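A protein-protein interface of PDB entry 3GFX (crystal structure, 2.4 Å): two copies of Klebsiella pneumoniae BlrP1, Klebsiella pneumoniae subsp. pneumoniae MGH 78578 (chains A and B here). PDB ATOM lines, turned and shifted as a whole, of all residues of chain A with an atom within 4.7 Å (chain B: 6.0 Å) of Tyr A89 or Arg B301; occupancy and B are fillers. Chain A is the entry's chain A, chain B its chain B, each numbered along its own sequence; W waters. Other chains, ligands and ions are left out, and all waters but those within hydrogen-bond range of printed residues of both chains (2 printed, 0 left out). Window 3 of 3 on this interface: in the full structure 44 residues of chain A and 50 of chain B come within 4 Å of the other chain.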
ATOM      1  N   MET A   9     -10.135 -32.881  18.533  1.00  0.00           N
ATOM      2  CA  MET A   9      -9.260 -32.285  19.589  1.00  0.00           C
ATOM      3  C   MET A   9      -9.546 -32.891  20.963  1.00  0.00           C
ATOM      4  O   MET A   9     -10.672 -32.818  21.465  1.00  0.00           O
ATOM      5  CB  MET A   9      -9.417 -30.761  19.627  1.00  0.00           C
ATOM      6  CG  MET A   9      -8.790 -30.040  18.438  1.00  0.00           C
ATOM      7  SD  MET A   9      -6.984 -30.078  18.453  1.00  0.00           S
ATOM      8  CE  MET A   9      -6.632 -28.892  19.749  1.00  0.00           C
ATOM      9  N   LEU A  10      -8.515 -33.483  21.557  1.00  0.00           N
ATOM     10  CA  LEU A  10      -8.640 -34.193  22.827  1.00  0.00           C
ATOM     11  C   LEU A  10      -8.864 -33.248  24.007  1.00  0.00           C
ATOM     12  O   LEU A  10      -8.264 -32.175  24.085  1.00  0.00           O
ATOM     13  CB  LEU A  10      -7.412 -35.077  23.067  1.00  0.00           C
ATOM     14  CG  LEU A  10      -7.485 -36.143  24.164  1.00  0.00           C
ATOM     15  CD1 LEU A  10      -8.616 -37.131  23.906  1.00  0.00           C
ATOM     16  CD2 LEU A  10      -6.163 -36.869  24.267  1.00  0.00           C
ATOM     17  N   THR A  11      -9.736 -33.670  24.918  1.00  0.00           N
ATOM     18  CA  THR A  11     -10.154 -32.863  26.059  1.00  0.00           C
ATOM     19  C   THR A  11     -10.191 -33.736  27.319  1.00  0.00           C
ATOM     20  O   THR A  11     -10.467 -34.932  27.245  1.00  0.00           O
ATOM     21  CB  THR A  11     -11.547 -32.216  25.785  1.00  0.00           C
ATOM     22  OG1 THR A  11     -11.463 -31.373  24.629  1.00  0.00           O
ATOM     23  CG2 THR A  11     -12.042 -31.385  26.967  1.00  0.00           C
ATOM     24  N   GLU A  63     -14.188 -32.681  22.741  1.00  0.00           N
ATOM     25  CA  GLU A  63     -14.993 -31.685  23.449  1.00  0.00           C
ATOM     26  C   GLU A  63     -16.493 -31.927  23.265  1.00  0.00           C
ATOM     27  O   GLU A  63     -17.278 -31.696  24.184  1.00  0.00           O
ATOM     28  CB  GLU A  63     -14.620 -30.271  22.989  1.00  0.00           C
ATOM     29  CG  GLU A  63     -15.199 -29.155  23.852  1.00  0.00           C
ATOM     30  CD  GLU A  63     -14.898 -27.770  23.306  1.00  0.00           C
ATOM     31  OE1 GLU A  63     -13.704 -27.440  23.129  1.00  0.00           O
ATOM     32  OE2 GLU A  63     -15.857 -27.005  23.060  1.00  0.00           O
ATOM     33  N   ASP A  88     -10.280 -29.006  30.181  1.00  0.00           N
ATOM     34  CA  ASP A  88      -9.224 -28.398  29.379  1.00  0.00           C
ATOM     35  C   ASP A  88      -8.785 -29.296  28.229  1.00  0.00           C
ATOM     36  O   ASP A  88      -9.028 -30.506  28.246  1.00  0.00           O
ATOM     37  CB  ASP A  88      -8.017 -28.075  30.264  1.00  0.00           C
ATOM     38  CG  ASP A  88      -7.303 -26.801  29.847  1.00  0.00           C
ATOM     39  OD1 ASP A  88      -7.200 -26.524  28.632  1.00  0.00           O
ATOM     40  OD2 ASP A  88      -6.836 -26.073  30.747  1.00  0.00           O
ATOM     41  N   TYR A  89      -8.133 -28.692  27.236  1.00  0.00           N
ATOM     42  CA  TYR A  89      -7.562 -29.425  26.111  1.00  0.00           C
ATOM     43  C   TYR A  89      -6.374 -30.268  26.572  1.00  0.00           C
ATOM     44  O   TYR A  89      -5.622 -29.861  27.460  1.00  0.00           O
ATOM     45  CB  TYR A  89      -7.147 -28.460  24.996  1.00  0.00           C
ATOM     46  CG  TYR A  89      -8.314 -27.752  24.339  1.00  0.00           C
ATOM     47  CD1 TYR A  89      -9.043 -28.365  23.320  1.00  0.00           C
ATOM     48  CD2 TYR A  89      -8.692 -26.474  24.739  1.00  0.00           C
ATOM     49  CE1 TYR A  89     -10.117 -27.722  22.717  1.00  0.00           C
ATOM     50  CE2 TYR A  89      -9.764 -25.823  24.144  1.00  0.00           C
ATOM     51  CZ  TYR A  89     -10.471 -26.450  23.133  1.00  0.00           C
ATOM     52  OH  TYR A  89     -11.533 -25.803  22.539  1.00  0.00           O
ATOM     53  N   SER A  90      -6.219 -31.445  25.973  1.00  0.00           N
ATOM     54  CA  SER A  90      -5.213 -32.404  26.414  1.00  0.00           C
ATOM     55  C   SER A  90      -4.200 -32.746  25.322  1.00  0.00           C
ATOM     56  O   SER A  90      -4.529 -32.769  24.135  1.00  0.00           O
ATOM     57  CB  SER A  90      -5.889 -33.676  26.933  1.00  0.00           C
ATOM     58  OG  SER A  90      -4.944 -34.572  27.487  1.00  0.00           O
ATOM     59  N   ALA A  91      -2.967 -33.012  25.746  1.00  0.00           N
ATOM     60  CA  ALA A  91      -1.884 -33.371  24.836  1.00  0.00           C
ATOM     61  C   ALA A  91      -1.971 -34.831  24.421  1.00  0.00           C
ATOM     62  O   ALA A  91      -1.729 -35.170  23.263  1.00  0.00           O
ATOM     63  CB  ALA A  91      -0.541 -33.099  25.486  1.00  0.00           C
ATOM     64  N   VAL B 296      -2.715 -19.003  23.099  1.00  0.00           N
ATOM     65  CA  VAL B 296      -1.325 -19.448  23.230  1.00  0.00           C
ATOM     66  C   VAL B 296      -1.182 -20.572  24.256  1.00  0.00           C
ATOM     67  O   VAL B 296      -0.462 -21.544  24.020  1.00  0.00           O
ATOM     68  CB  VAL B 296      -0.366 -18.257  23.523  1.00  0.00           C
ATOM     69  CG1 VAL B 296       0.877 -18.702  24.292  1.00  0.00           C
ATOM     70  CG2 VAL B 296       0.046 -17.616  22.216  1.00  0.00           C
ATOM     71  N   LEU B 297      -1.891 -20.442  25.375  1.00  0.00           N
ATOM     72  CA  LEU B 297      -1.904 -21.467  26.415  1.00  0.00           C
ATOM     73  C   LEU B 297      -2.491 -22.777  25.883  1.00  0.00           C
ATOM     74  O   LEU B 297      -1.988 -23.853  26.202  1.00  0.00           O
ATOM     75  CB  LEU B 297      -2.677 -20.970  27.646  1.00  0.00           C
ATOM     76  CG  LEU B 297      -2.631 -21.713  28.992  1.00  0.00           C
ATOM     77  CD1 LEU B 297      -3.786 -22.695  29.131  1.00  0.00           C
ATOM     78  CD2 LEU B 297      -1.288 -22.399  29.257  1.00  0.00           C
ATOM     79  N   LYS B 298      -3.540 -22.669  25.069  1.00  0.00           N
ATOM     80  CA  LYS B 298      -4.161 -23.826  24.420  1.00  0.00           C
ATOM     81  C   LYS B 298      -3.159 -24.573  23.543  1.00  0.00           C
ATOM     82  O   LYS B 298      -3.059 -25.798  23.616  1.00  0.00           O
ATOM     83  CB  LYS B 298      -5.373 -23.391  23.590  1.00  0.00           C
ATOM     84  CG  LYS B 298      -6.078 -24.518  22.847  1.00  0.00           C
ATOM     85  CD  LYS B 298      -7.279 -23.994  22.073  1.00  0.00           C
ATOM     86  CE  LYS B 298      -7.806 -25.027  21.090  1.00  0.00           C
ATOM     87  NZ  LYS B 298      -6.867 -25.239  19.951  1.00  0.00           N
ATOM     88  N   ALA B 299      -2.411 -23.825  22.734  1.00  0.00           N
ATOM     89  CA  ALA B 299      -1.389 -24.399  21.863  1.00  0.00           C
ATOM     90  C   ALA B 299      -0.252 -25.050  22.653  1.00  0.00           C
ATOM     91  O   ALA B 299       0.311 -26.052  22.217  1.00  0.00           O
ATOM     92  CB  ALA B 299      -0.849 -23.342  20.912  1.00  0.00           C
ATOM     93  N   LEU B 300       0.070 -24.480  23.815  1.00  0.00           N
ATOM     94  CA  LEU B 300       1.079 -25.044  24.715  1.00  0.00           C
ATOM     95  C   LEU B 300       0.613 -26.350  25.356  1.00  0.00           C
ATOM     96  O   LEU B 300       1.381 -27.310  25.437  1.00  0.00           O
ATOM     97  CB  LEU B 300       1.452 -24.044  25.813  1.00  0.00           C
ATOM     98  CG  LEU B 300       2.278 -22.809  25.445  1.00  0.00           C
ATOM     99  CD1 LEU B 300       2.308 -21.831  26.609  1.00  0.00           C
ATOM    100  CD2 LEU B 300       3.691 -23.185  25.018  1.00  0.00           C
ATOM    101  N   ARG B 301      -0.640 -26.365  25.810  1.00  0.00           N
ATOM    102  CA  ARG B 301      -1.253 -27.540  26.437  1.00  0.00           C
ATOM    103  C   ARG B 301      -1.278 -28.736  25.494  1.00  0.00           C
ATOM    104  O   ARG B 301      -0.815 -29.819  25.850  1.00  0.00           O
ATOM    105  CB  ARG B 301      -2.685 -27.228  26.891  1.00  0.00           C
ATOM    106  CG  ARG B 301      -2.789 -26.376  28.143  1.00  0.00           C
ATOM    107  CD  ARG B 301      -2.790 -27.212  29.412  1.00  0.00           C
ATOM    108  NE  ARG B 301      -2.188 -26.486  30.527  1.00  0.00           N
ATOM    109  CZ  ARG B 301      -2.843 -25.660  31.341  1.00  0.00           C
ATOM    110  NH1 ARG B 301      -4.143 -25.441  31.183  1.00  0.00           N
ATOM    111  NH2 ARG B 301      -2.192 -25.053  32.319  1.00  0.00           N
ATOM    112  N   VAL B 302      -1.817 -28.520  24.296  1.00  0.00           N
ATOM    113  CA  VAL B 302      -1.967 -29.565  23.280  1.00  0.00           C
ATOM    114  C   VAL B 302      -0.614 -30.105  22.808  1.00  0.00           C
ATOM    115  O   VAL B 302      -0.467 -31.305  22.566  1.00  0.00           O
ATOM    116  CB  VAL B 302      -2.821 -29.058  22.085  1.00  0.00           C
ATOM    117  CG1 VAL B 302      -2.921 -30.105  20.978  1.00  0.00           C
ATOM    118  CG2 VAL B 302      -4.209 -28.672  22.564  1.00  0.00           C
ATOM    119  N   ALA B 303       0.374 -29.219  22.701  1.00  0.00           N
ATOM    120  CA  ALA B 303       1.734 -29.616  22.342  1.00  0.00           C
ATOM    121  C   ALA B 303       2.388 -30.457  23.437  1.00  0.00           C
ATOM    122  O   ALA B 303       3.227 -31.312  23.153  1.00  0.00           O
ATOM    123  CB  ALA B 303       2.582 -28.393  22.033  1.00  0.00           C
ATOM    124  N   GLY B 304       1.998 -30.209  24.684  1.00  0.00           N
ATOM    125  CA  GLY B 304       2.502 -30.975  25.819  1.00  0.00           C
ATOM    126  C   GLY B 304       3.361 -30.167  26.768  1.00  0.00           C
ATOM    127  O   GLY B 304       3.811 -30.679  27.792  1.00  0.00           O
ATOM    128  N   MET B 305       3.587 -28.902  26.433  1.00  0.00           N
ATOM    129  CA  MET B 305       4.409 -28.025  27.259  1.00  0.00           C
ATOM    130  C   MET B 305       3.658 -27.504  28.479  1.00  0.00           C
ATOM    131  O   MET B 305       2.426 -27.456  28.496  1.00  0.00           O
ATOM    132  CB  MET B 305       4.968 -26.870  26.430  1.00  0.00           C
ATOM    133  CG  MET B 305       6.134 -27.272  25.540  1.00  0.00           C
ATOM    134  SD  MET B 305       6.697 -25.941  24.467  1.00  0.00           S
ATOM    135  CE  MET B 305       5.445 -25.984  23.190  1.00  0.00           C
ATOM    136  N   LEU B 307       3.157 -24.559  31.797  1.00  0.00           N
ATOM    137  CA  LEU B 307       3.190 -23.121  32.048  1.00  0.00           C
ATOM    138  C   LEU B 307       3.100 -22.792  33.534  1.00  0.00           C
ATOM    139  O   LEU B 307       2.338 -23.417  34.274  1.00  0.00           O
ATOM    140  CB  LEU B 307       2.094 -22.398  31.254  1.00  0.00           C
ATOM    141  CG  LEU B 307       2.013 -20.872  31.392  1.00  0.00           C
ATOM    142  CD1 LEU B 307       2.066 -20.194  30.034  1.00  0.00           C
ATOM    143  CD2 LEU B 307       0.778 -20.447  32.176  1.00  0.00           C
ATOM    144  N   PHE B 325      -7.974 -19.262  33.688  1.00  0.00           N
ATOM    145  CA  PHE B 325      -7.187 -20.427  33.305  1.00  0.00           C
ATOM    146  C   PHE B 325      -6.431 -20.944  34.520  1.00  0.00           C
ATOM    147  O   PHE B 325      -6.227 -20.211  35.489  1.00  0.00           O
ATOM    148  CB  PHE B 325      -6.196 -20.077  32.183  1.00  0.00           C
ATOM    149  CG  PHE B 325      -5.136 -19.083  32.590  1.00  0.00           C
ATOM    150  CD1 PHE B 325      -5.356 -17.717  32.452  1.00  0.00           C
ATOM    151  CD2 PHE B 325      -3.915 -19.515  33.103  1.00  0.00           C
ATOM    152  CE1 PHE B 325      -4.385 -16.800  32.827  1.00  0.00           C
ATOM    153  CE2 PHE B 325      -2.941 -18.606  33.481  1.00  0.00           C
ATOM    154  CZ  PHE B 325      -3.174 -17.247  33.343  1.00  0.00           C
ATOM    155  N   GLN B 326      -6.001 -22.199  34.461  1.00  0.00           N
ATOM    156  CA  GLN B 326      -5.193 -22.770  35.526  1.00  0.00           C
ATOM    157  C   GLN B 326      -3.833 -23.184  34.978  1.00  0.00           C
ATOM    158  O   GLN B 326      -3.757 -24.029  34.084  1.00  0.00           O
ATOM    159  CB  GLN B 326      -5.897 -23.963  36.180  1.00  0.00           C
ATOM    160  CG  GLN B 326      -7.240 -23.633  36.830  1.00  0.00           C
ATOM    161  CD  GLN B 326      -8.401 -23.692  35.852  1.00  0.00           C
ATOM    162  OE1 GLN B 326      -8.506 -24.617  35.046  1.00  0.00           O
ATOM    163  NE2 GLN B 326      -9.281 -22.702  35.922  1.00  0.00           N
ATOM    164  N   PRO B 327      -2.753 -22.573  35.497  1.00  0.00           N
ATOM    165  CA  PRO B 327      -1.399 -22.980  35.146  1.00  0.00           C
ATOM    166  C   PRO B 327      -1.022 -24.284  35.844  1.00  0.00           C
ATOM    167  O   PRO B 327      -1.719 -24.727  36.760  1.00  0.00           O
ATOM    168  CB  PRO B 327      -0.544 -21.831  35.685  1.00  0.00           C
ATOM    169  CG  PRO B 327      -1.313 -21.319  36.841  1.00  0.00           C
ATOM    170  CD  PRO B 327      -2.757 -21.444  36.444  1.00  0.00           C
ATOM    171  N   ASP B 328       0.080 -24.886  35.412  1.00  0.00           N
ATOM    172  CA  ASP B 328       0.586 -26.100  36.037  1.00  0.00           C
ATOM    173  C   ASP B 328       1.304 -25.773  37.341  1.00  0.00           C
ATOM    174  O   ASP B 328       1.383 -26.608  38.243  1.00  0.00           O
ATOM    175  CB  ASP B 328       1.528 -26.827  35.079  1.00  0.00           C
ATOM    176  CG  ASP B 328       0.842 -27.230  33.790  1.00  0.00           C
ATOM    177  OD1 ASP B 328       0.069 -28.208  33.806  1.00  0.00           O
ATOM    178  OD2 ASP B 328       1.076 -26.566  32.760  1.00  0.00           O
HETATM  179  O   HOH W   1      -6.776 -23.520  31.830  1.00  0.00           O
HETATM  180  O   HOH W   2      -1.057 -33.557  21.036  1.00  0.00           O
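NH1 of Arg B301 is in salt-bridge range of OD2 of Asp A88 (2.8 Å).
The side-chain hydroxyl (OH) of Tyr A89 is in hydrogen-bond range of the side-chain carboxylate (OE1) of Glu A63, 2.8 Å away. O of Gln B326 lies within hydrogen-bond range of NH2 of Arg B301 (2.6 Å). The guanidinium group of Arg B301 is in salt-bridge range of the side-chain carboxylate of Asp B328, at 3.6 Å.
CE of Met A9 touches NZ of Lys B298 (3.7 Å). CG2 of Val B302 touches CE of Met A9 (3.7 Å). Tyr A89 touches Lys B298. Arg B301 touches Tyr A89 (CB to O, 3.99 Å). Tyr A89 touches Val B302 (CB to CG2, 3.8 Å). Ala A91 touches Arg B301 (CB to O, 3.3 Å). Ala A91 touches Val B302 (CA to O, 3.4 Å). CB of Ala A91 touches CA of Gly B304, 3.7 Å away.
Of the printed residues of chain B, Met A9 touches Lys B298 (3.7 Å) and Val B302 (3.7 Å). Printed residues of chain B within 4 Å of Asp A88: Arg B301 (2.8 Å). Of the printed residues of chain B, Tyr A89 touches Lys B298, Arg B301 and Val B302. Of the printed residues of chain B, Ala A91 touches Arg B301 (3.3 Å), Val B302 (3.4 Å) and Gly B304 (3.7 Å). Of the printed residues of chain A, Arg B301 touches Asp A88, Tyr A89 and Ala A91. Of the printed residues of chain A, Gly B304 touches Ala A91 (3.7 Å).
Of the 15 printed residues of chain B, 4 touch a printed residue of chain A. Printed residues of chain B that touch a printed residue of chain A: Lys B298, Arg B301, Val B302 and Gly B304.
No position is printed for both chains. Of the 9 pairs that touch across the chains among the printed residues, none has its exchanged pair printed and touching as well.
Water W1 lies within hydrogen-bond range of OD2 of Asp A88 (2.8 Å), N of Gln B326 (3.0 Å) and NH1 of Arg B301 (3.3 Å). Water W2 bridges O of Val B302 and O of Ala A91.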
